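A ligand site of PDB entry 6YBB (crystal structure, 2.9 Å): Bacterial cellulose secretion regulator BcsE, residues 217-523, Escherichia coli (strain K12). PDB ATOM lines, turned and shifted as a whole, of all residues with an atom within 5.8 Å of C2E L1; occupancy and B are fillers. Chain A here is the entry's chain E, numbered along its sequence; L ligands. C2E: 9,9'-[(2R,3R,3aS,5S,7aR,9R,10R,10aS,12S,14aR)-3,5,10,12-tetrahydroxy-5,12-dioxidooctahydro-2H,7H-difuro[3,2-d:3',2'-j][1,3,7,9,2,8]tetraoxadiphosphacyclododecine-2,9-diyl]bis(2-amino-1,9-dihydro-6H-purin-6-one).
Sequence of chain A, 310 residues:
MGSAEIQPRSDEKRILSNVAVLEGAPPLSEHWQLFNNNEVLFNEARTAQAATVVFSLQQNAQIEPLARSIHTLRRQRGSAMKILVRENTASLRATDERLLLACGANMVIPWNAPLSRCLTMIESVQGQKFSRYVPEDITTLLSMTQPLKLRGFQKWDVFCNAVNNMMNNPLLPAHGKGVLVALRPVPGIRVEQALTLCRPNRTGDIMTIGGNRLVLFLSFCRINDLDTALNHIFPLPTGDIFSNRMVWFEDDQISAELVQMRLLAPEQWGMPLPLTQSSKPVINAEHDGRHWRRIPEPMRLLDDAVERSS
The backbone carbonyl oxygen of Leu 92 lies close to an oxygen (O1P) of C2E L1. NH2 of Arg 202 is in salt-bridge range of O2P of C2E L1. The guanidinium group (NH2) of Arg 93 is in hydrogen-bond range of an oxygen (O6) of C2E L1, at 2.9 Å. An oxygen (O2P) of C2E L2 lies within salt-bridge range of the guanidinium group (NH2) of Arg 93 (2.6 Å). An oxygen (O4') of C2E L1 sits at hydrogen-bond distance from the backbone NH (N) of Leu 92, 3.1 Å away. N21 of C2E L1 lies within hydrogen-bond range of OD2 of Asp 205 (3.4 Å). A nitrogen (N71) of C2E L2 sits at hydrogen-bond distance from the side-chain amide nitrogen (ND2) of Asn 60 (3.1 Å). NH2 of Arg 202 is in hydrogen-bond range of O6 of C2E L2.
Residues that only touch C2E L1: Ala 90 (3.6 Å), Ser 91 (3.0 Å), Asn 201 (3.7 Å), Thr 228 (3.2 Å), Ala 229 (3.4 Å) and His 232 (3.4 Å). Hydrophobic or aromatic side chains that line C2E L1: Ala 229 and His 232. Within 4 Å of C2E L1: Ala 90, Ser 91, Leu 92, Arg 93, Asn 201, Arg 202, Asp 205, Thr 228, Ala 229 and His 232. The nearest printed residue that does not touch C2E L1 is Asp 225 (4.1 Å).
The backbone carbonyl oxygen (O) of Thr 228 is in hydrogen-bond range of a ring nitrogen (ND1) of His 232, at 2.7 Å.
A nitrogen (N1) of C2E L1 is in hydrogen-bond range of an oxygen (O21) of C2E L2 (2.5 Å).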
ATOM      1  N   ASN A  60       1.629  32.860   0.561  1.00  0.00           N
ATOM      2  CA  ASN A  60       2.949  32.893   1.179  1.00  0.00           C
ATOM      3  C   ASN A  60       3.156  34.128   2.029  1.00  0.00           C
ATOM      4  O   ASN A  60       4.062  34.156   2.862  1.00  0.00           O
ATOM      5  CB  ASN A  60       4.031  32.800   0.104  1.00  0.00           C
ATOM      6  CG  ASN A  60       3.757  33.704  -1.078  1.00  0.00           C
ATOM      7  OD1 ASN A  60       3.104  34.735  -0.953  1.00  0.00           O
ATOM      8  ND2 ASN A  60       4.255  33.313  -2.252  1.00  0.00           N
ATOM      9  N   ALA A  90      -0.577  25.561  -3.575  1.00  0.00           N
ATOM     10  CA  ALA A  90       0.679  24.916  -3.927  1.00  0.00           C
ATOM     11  C   ALA A  90       1.850  25.887  -3.893  1.00  0.00           C
ATOM     12  O   ALA A  90       3.004  25.450  -4.023  1.00  0.00           O
ATOM     13  CB  ALA A  90       0.578  24.272  -5.307  1.00  0.00           C
ATOM     14  N   SER A  91       1.598  27.193  -3.714  1.00  0.00           N
ATOM     15  CA  SER A  91       2.649  28.210  -3.742  1.00  0.00           C
ATOM     16  C   SER A  91       3.285  28.307  -2.368  1.00  0.00           C
ATOM     17  O   SER A  91       2.925  29.127  -1.522  1.00  0.00           O
ATOM     18  CB  SER A  91       2.086  29.560  -4.177  1.00  0.00           C
ATOM     19  OG  SER A  91       1.319  29.440  -5.361  1.00  0.00           O
ATOM     20  N   LEU A  92       4.268  27.443  -2.132  1.00  0.00           N
ATOM     21  CA  LEU A  92       4.836  27.317  -0.808  1.00  0.00           C
ATOM     22  C   LEU A  92       6.151  26.563  -0.897  1.00  0.00           C
ATOM     23  O   LEU A  92       6.208  25.480  -1.493  1.00  0.00           O
ATOM     24  CB  LEU A  92       3.872  26.575   0.118  1.00  0.00           C
ATOM     25  CG  LEU A  92       3.807  27.099   1.546  1.00  0.00           C
ATOM     26  CD1 LEU A  92       3.015  28.385   1.561  1.00  0.00           C
ATOM     27  CD2 LEU A  92       3.182  26.048   2.439  1.00  0.00           C
ATOM     28  N   ARG A  93       7.203  27.123  -0.311  1.00  0.00           N
ATOM     29  CA  ARG A  93       8.510  26.495  -0.255  1.00  0.00           C
ATOM     30  C   ARG A  93       8.580  25.467   0.865  1.00  0.00           C
ATOM     31  O   ARG A  93       7.868  25.550   1.871  1.00  0.00           O
ATOM     32  CB  ARG A  93       9.597  27.551  -0.046  1.00  0.00           C
ATOM     33  CG  ARG A  93       9.773  28.530  -1.195  1.00  0.00           C
ATOM     34  CD  ARG A  93      10.954  29.438  -0.967  1.00  0.00           C
ATOM     35  NE  ARG A  93      10.984  30.542  -1.929  1.00  0.00           N
ATOM     36  CZ  ARG A  93      11.948  31.448  -1.987  1.00  0.00           C
ATOM     37  NH1 ARG A  93      12.975  31.387  -1.154  1.00  0.00           N
ATOM     38  NH2 ARG A  93      11.889  32.423  -2.901  1.00  0.00           N
ATOM     39  N   ALA A  94       9.477  24.496   0.694  1.00  0.00           N
ATOM     40  CA  ALA A  94       9.647  23.414   1.665  1.00  0.00           C
ATOM     41  C   ALA A  94      10.234  23.889   2.987  1.00  0.00           C
ATOM     42  O   ALA A  94      10.017  23.236   4.012  1.00  0.00           O
ATOM     43  CB  ALA A  94      10.543  22.317   1.080  1.00  0.00           C
ATOM     44  N   ASN A 201      17.325  33.505  -9.708  1.00  0.00           N
ATOM     45  CA  ASN A 201      16.317  34.455  -9.277  1.00  0.00           C
ATOM     46  C   ASN A 201      16.275  34.642  -7.768  1.00  0.00           C
ATOM     47  O   ASN A 201      16.058  35.769  -7.294  1.00  0.00           O
ATOM     48  CB  ASN A 201      14.932  34.015  -9.768  1.00  0.00           C
ATOM     49  CG  ASN A 201      14.860  33.878 -11.269  1.00  0.00           C
ATOM     50  OD1 ASN A 201      15.381  34.724 -11.996  1.00  0.00           O
ATOM     51  ND2 ASN A 201      14.233  32.815 -11.733  1.00  0.00           N
ATOM     52  N   ARG A 202      16.475  33.571  -7.019  1.00  0.00           N
ATOM     53  CA  ARG A 202      16.322  33.605  -5.572  1.00  0.00           C
ATOM     54  C   ARG A 202      17.509  34.300  -4.903  1.00  0.00           C
ATOM     55  O   ARG A 202      18.668  34.094  -5.284  1.00  0.00           O
ATOM     56  CB  ARG A 202      16.194  32.194  -5.008  1.00  0.00           C
ATOM     57  CG  ARG A 202      14.853  31.535  -5.259  1.00  0.00           C
ATOM     58  CD  ARG A 202      14.740  30.211  -4.530  1.00  0.00           C
ATOM     59  NE  ARG A 202      13.416  29.615  -4.664  1.00  0.00           N
ATOM     60  CZ  ARG A 202      13.048  28.484  -4.075  1.00  0.00           C
ATOM     61  NH1 ARG A 202      13.909  27.840  -3.297  1.00  0.00           N
ATOM     62  NH2 ARG A 202      11.820  28.008  -4.251  1.00  0.00           N
ATOM     63  N   ASP A 205      21.050  32.268  -3.759  1.00  0.00           N
ATOM     64  CA  ASP A 205      21.669  31.452  -4.792  1.00  0.00           C
ATOM     65  C   ASP A 205      22.835  32.240  -5.369  1.00  0.00           C
ATOM     66  O   ASP A 205      22.636  33.263  -6.037  1.00  0.00           O
ATOM     67  CB  ASP A 205      20.649  31.083  -5.879  1.00  0.00           C
ATOM     68  CG  ASP A 205      19.507  30.224  -5.359  1.00  0.00           C
ATOM     69  OD1 ASP A 205      19.544  29.809  -4.181  1.00  0.00           O
ATOM     70  OD2 ASP A 205      18.564  29.967  -6.138  1.00  0.00           O
ATOM     71  N   LEU A 218      23.187  26.765  -3.597  1.00  0.00           N
ATOM     72  CA  LEU A 218      21.751  27.005  -3.604  1.00  0.00           C
ATOM     73  C   LEU A 218      21.264  26.866  -2.169  1.00  0.00           C
ATOM     74  O   LEU A 218      21.181  25.754  -1.643  1.00  0.00           O
ATOM     75  CB  LEU A 218      21.046  26.023  -4.540  1.00  0.00           C
ATOM     76  CG  LEU A 218      21.781  25.749  -5.846  1.00  0.00           C
ATOM     77  CD1 LEU A 218      21.012  24.730  -6.689  1.00  0.00           C
ATOM     78  CD2 LEU A 218      22.017  27.042  -6.628  1.00  0.00           C
ATOM     79  N   CYS A 221      18.393  24.286  -0.509  1.00  0.00           N
ATOM     80  CA  CYS A 221      17.981  23.372  -1.566  1.00  0.00           C
ATOM     81  C   CYS A 221      18.218  21.929  -1.127  1.00  0.00           C
ATOM     82  O   CYS A 221      19.295  21.606  -0.622  1.00  0.00           O
ATOM     83  CB  CYS A 221      18.736  23.658  -2.861  1.00  0.00           C
ATOM     84  SG  CYS A 221      18.424  22.446  -4.164  1.00  0.00           S
ATOM     85  N   ASP A 225      15.579  18.178  -5.034  1.00  0.00           N
ATOM     86  CA  ASP A 225      15.205  19.367  -5.814  1.00  0.00           C
ATOM     87  C   ASP A 225      16.375  19.966  -6.590  1.00  0.00           C
ATOM     88  O   ASP A 225      16.167  21.022  -7.201  1.00  0.00           O
ATOM     89  CB  ASP A 225      14.617  20.428  -4.892  1.00  0.00           C
ATOM     90  CG  ASP A 225      13.521  19.884  -4.005  1.00  0.00           C
ATOM     91  OD1 ASP A 225      13.210  18.676  -4.122  1.00  0.00           O
ATOM     92  OD2 ASP A 225      12.975  20.652  -3.182  1.00  0.00           O
ATOM     93  N   THR A 228      15.556  20.257 -10.371  1.00  0.00           N
ATOM     94  CA  THR A 228      14.489  21.231 -10.589  1.00  0.00           C
ATOM     95  C   THR A 228      15.008  22.652 -10.435  1.00  0.00           C
ATOM     96  O   THR A 228      14.670  23.540 -11.228  1.00  0.00           O
ATOM     97  CB  THR A 228      13.351  20.980  -9.602  1.00  0.00           C
ATOM     98  OG1 THR A 228      12.984  19.595  -9.629  1.00  0.00           O
ATOM     99  CG2 THR A 228      12.143  21.838  -9.960  1.00  0.00           C
ATOM    100  N   ALA A 229      15.832  22.897  -9.404  1.00  0.00           N
ATOM    101  CA  ALA A 229      16.385  24.231  -9.193  1.00  0.00           C
ATOM    102  C   ALA A 229      17.370  24.596 -10.298  1.00  0.00           C
ATOM    103  O   ALA A 229      17.381  25.740 -10.755  1.00  0.00           O
ATOM    104  CB  ALA A 229      17.049  24.308  -7.821  1.00  0.00           C
ATOM    105  N   HIS A 232      15.661  25.881 -13.277  1.00  0.00           N
ATOM    106  CA  HIS A 232      15.231  27.255 -13.106  1.00  0.00           C
ATOM    107  C   HIS A 232      16.380  28.246 -13.078  1.00  0.00           C
ATOM    108  O   HIS A 232      16.137  29.463 -13.125  1.00  0.00           O
ATOM    109  CB  HIS A 232      14.395  27.398 -11.829  1.00  0.00           C
ATOM    110  CG  HIS A 232      13.025  26.804 -11.923  1.00  0.00           C
ATOM    111  ND1 HIS A 232      12.783  25.457 -11.757  1.00  0.00           N
ATOM    112  CD2 HIS A 232      11.827  27.375 -12.199  1.00  0.00           C
ATOM    113  CE1 HIS A 232      11.492  25.222 -11.915  1.00  0.00           C
ATOM    114  NE2 HIS A 232      10.888  26.368 -12.182  1.00  0.00           N
ATOM    115  N   ILE A 233      17.632  27.778 -12.996  1.00  0.00           N
ATOM    116  CA  ILE A 233      18.780  28.674 -13.056  1.00  0.00           C
ATOM    117  C   ILE A 233      19.267  28.833 -14.492  1.00  0.00           C
ATOM    118  O   ILE A 233      19.542  29.959 -14.937  1.00  0.00           O
ATOM    119  CB  ILE A 233      19.917  28.178 -12.131  1.00  0.00           C
ATOM    120  CG1 ILE A 233      19.430  27.989 -10.694  1.00  0.00           C
ATOM    121  CG2 ILE A 233      21.076  29.156 -12.146  1.00  0.00           C
ATOM    122  CD1 ILE A 233      18.917  29.251 -10.029  1.00  0.00           C
HETATM  123  P1  C2E L   1       8.823  24.990  -4.076  1.00  0.00           P
HETATM  124  O2P C2E L   1      10.107  25.485  -3.437  1.00  0.00           O
HETATM  125  O1P C2E L   1       7.984  24.167  -3.187  1.00  0.00           O
HETATM  126  O5' C2E L   1       8.034  26.253  -4.658  1.00  0.00           O
HETATM  127  C5' C2E L   1       6.660  26.487  -4.301  1.00  0.00           C
HETATM  128  C4' C2E L   1       5.898  27.191  -5.389  1.00  0.00           C
HETATM  129  O4' C2E L   1       5.373  28.428  -4.864  1.00  0.00           O
HETATM  130  C3' C2E L   1       6.699  27.589  -6.635  1.00  0.00           C
HETATM  131  O3' C2E L   1       6.547  26.589  -7.656  1.00  0.00           O
HETATM  132  C2' C2E L   1       5.985  28.857  -7.103  1.00  0.00           C
HETATM  133  O2' C2E L   1       4.781  28.522  -7.784  1.00  0.00           O
HETATM  134  C1' C2E L   1       5.657  29.497  -5.755  1.00  0.00           C
HETATM  135  N9  C2E L   1       6.756  30.287  -5.189  1.00  0.00           N
HETATM  136  C8  C2E L   1       7.642  29.911  -4.203  1.00  0.00           C
HETATM  137  N7  C2E L   1       8.511  30.849  -3.899  1.00  0.00           N
HETATM  138  C5  C2E L   1       8.175  31.906  -4.734  1.00  0.00           C
HETATM  139  C6  C2E L   1       8.755  33.216  -4.865  1.00  0.00           C
HETATM  140  O6  C2E L   1       9.710  33.677  -4.252  1.00  0.00           O
HETATM  141  N1  C2E L   1       8.098  33.966  -5.815  1.00  0.00           N
HETATM  142  C2  C2E L   1       7.037  33.539  -6.570  1.00  0.00           C
HETATM  143  N2  C2E L   1       6.542  34.402  -7.454  1.00  0.00           N
HETATM  144  N3  C2E L   1       6.492  32.338  -6.452  1.00  0.00           N
HETATM  145  C4  C2E L   1       7.104  31.578  -5.526  1.00  0.00           C
HETATM  146  P11 C2E L   1       7.050  26.485  -9.161  1.00  0.00           P
HETATM  147  O21 C2E L   1       7.483  27.870  -9.652  1.00  0.00           O
HETATM  148  O11 C2E L   1       6.044  25.824 -10.032  1.00  0.00           O
HETATM  149  O5A C2E L   1       8.379  25.579  -9.026  1.00  0.00           O
HETATM  150  C5A C2E L   1       8.424  24.205  -8.593  1.00  0.00           C
HETATM  151  C4A C2E L   1       9.694  23.983  -7.825  1.00  0.00           C
HETATM  152  O4A C2E L   1      10.820  24.432  -8.619  1.00  0.00           O
HETATM  153  C3A C2E L   1       9.827  24.813  -6.555  1.00  0.00           C
HETATM  154  O3A C2E L   1       9.181  24.232  -5.408  1.00  0.00           O
HETATM  155  C2A C2E L   1      11.338  24.843  -6.337  1.00  0.00           C
HETATM  156  O2A C2E L   1      11.801  23.638  -5.743  1.00  0.00           O
HETATM  157  C1A C2E L   1      11.824  24.991  -7.787  1.00  0.00           C
HETATM  158  N91 C2E L   1      12.039  26.399  -8.173  1.00  0.00           N
HETATM  159  C81 C2E L   1      11.174  27.228  -8.831  1.00  0.00           C
HETATM  160  N71 C2E L   1      11.649  28.436  -9.020  1.00  0.00           N
HETATM  161  C51 C2E L   1      12.922  28.396  -8.451  1.00  0.00           C
HETATM  162  C61 C2E L   1      13.950  29.399  -8.342  1.00  0.00           C
HETATM  163  O61 C2E L   1      13.921  30.553  -8.768  1.00  0.00           O
HETATM  164  N11 C2E L   1      15.069  28.922  -7.693  1.00  0.00           N
HETATM  165  C21 C2E L   1      15.219  27.651  -7.188  1.00  0.00           C
HETATM  166  N21 C2E L   1      16.356  27.383  -6.556  1.00  0.00           N
HETATM  167  N31 C2E L   1      14.269  26.710  -7.286  1.00  0.00           N
HETATM  168  C41 C2E L   1      13.167  27.138  -7.920  1.00  0.00           C
HETATM  169  P1  C2E L   2      13.542  35.848  -3.951  1.00  0.00           P
HETATM  170  O2P C2E L   2      13.541  34.428  -3.398  1.00  0.00           O
HETATM  171  O1P C2E L   2      14.869  36.506  -4.011  1.00  0.00           O
HETATM  172  O5' C2E L   2      12.851  35.768  -5.384  1.00  0.00           O
HETATM  173  C5' C2E L   2      12.909  36.853  -6.348  1.00  0.00           C
HETATM  174  C4' C2E L   2      11.889  36.614  -7.426  1.00  0.00           C
HETATM  175  O4' C2E L   2      12.261  35.476  -8.226  1.00  0.00           O
HETATM  176  C3' C2E L   2      10.495  36.253  -6.924  1.00  0.00           C
HETATM  177  O3' C2E L   2       9.718  37.430  -6.593  1.00  0.00           O
HETATM  178  C2' C2E L   2       9.897  35.561  -8.143  1.00  0.00           C
HETATM  179  O2' C2E L   2       9.492  36.512  -9.124  1.00  0.00           O
HETATM  180  C1' C2E L   2      11.107  34.752  -8.619  1.00  0.00           C
HETATM  181  N9  C2E L   2      11.163  33.425  -7.983  1.00  0.00           N
HETATM  182  C8  C2E L   2      12.077  32.966  -7.074  1.00  0.00           C
HETATM  183  N7  C2E L   2      11.803  31.760  -6.626  1.00  0.00           N
HETATM  184  C5  C2E L   2      10.643  31.406  -7.296  1.00  0.00           C
HETATM  185  C6  C2E L   2       9.825  30.232  -7.212  1.00  0.00           C
HETATM  186  O6  C2E L   2      10.012  29.239  -6.516  1.00  0.00           O
HETATM  187  N1  C2E L   2       8.734  30.303  -8.047  1.00  0.00           N
HETATM  188  C2  C2E L   2       8.421  31.350  -8.862  1.00  0.00           C
HETATM  189  N2  C2E L   2       7.325  31.244  -9.605  1.00  0.00           N
HETATM  190  N3  C2E L   2       9.162  32.453  -8.944  1.00  0.00           N
HETATM  191  C4  C2E L   2      10.243  32.422  -8.145  1.00  0.00           C
HETATM  192  P11 C2E L   2       8.469  37.568  -5.633  1.00  0.00           P
HETATM  193  O21 C2E L   2       7.550  36.398  -5.959  1.00  0.00           O
HETATM  194  O11 C2E L   2       7.863  38.909  -5.765  1.00  0.00           O
HETATM  195  O5A C2E L   2       9.032  37.329  -4.140  1.00  0.00           O
HETATM  196  C5A C2E L   2       9.691  38.316  -3.321  1.00  0.00           C
HETATM  197  C4A C2E L   2      10.428  37.653  -2.190  1.00  0.00           C
HETATM  198  O4A C2E L   2       9.476  37.174  -1.197  1.00  0.00           O
HETATM  199  C3A C2E L   2      11.216  36.404  -2.561  1.00  0.00           C
HETATM  200  O3A C2E L   2      12.524  36.714  -3.082  1.00  0.00           O
HETATM  201  C2A C2E L   2      11.312  35.675  -1.220  1.00  0.00           C
HETATM  202  O2A C2E L   2      12.301  36.275  -0.388  1.00  0.00           O
HETATM  203  C1A C2E L   2       9.913  35.937  -0.663  1.00  0.00           C
HETATM  204  N91 C2E L   2       8.939  34.904  -1.039  1.00  0.00           N
HETATM  205  C81 C2E L   2       8.036  34.959  -2.068  1.00  0.00           C
HETATM  206  N71 C2E L   2       7.324  33.867  -2.210  1.00  0.00           N
HETATM  207  C51 C2E L   2       7.782  33.039  -1.189  1.00  0.00           C
HETATM  208  C61 C2E L   2       7.395  31.699  -0.818  1.00  0.00           C
HETATM  209  O61 C2E L   2       6.567  30.981  -1.369  1.00  0.00           O
HETATM  210  N11 C2E L   2       8.100  31.246   0.280  1.00  0.00           N
HETATM  211  C21 C2E L   2       9.060  31.959   0.954  1.00  0.00           C
HETATM  212  N21 C2E L   2       9.619  31.373   2.013  1.00  0.00           N
HETATM  213  N31 C2E L   2       9.435  33.189   0.602  1.00  0.00           N
HETATM  214  C41 C2E L   2       8.768  33.664  -0.464  1.00  0.00           C
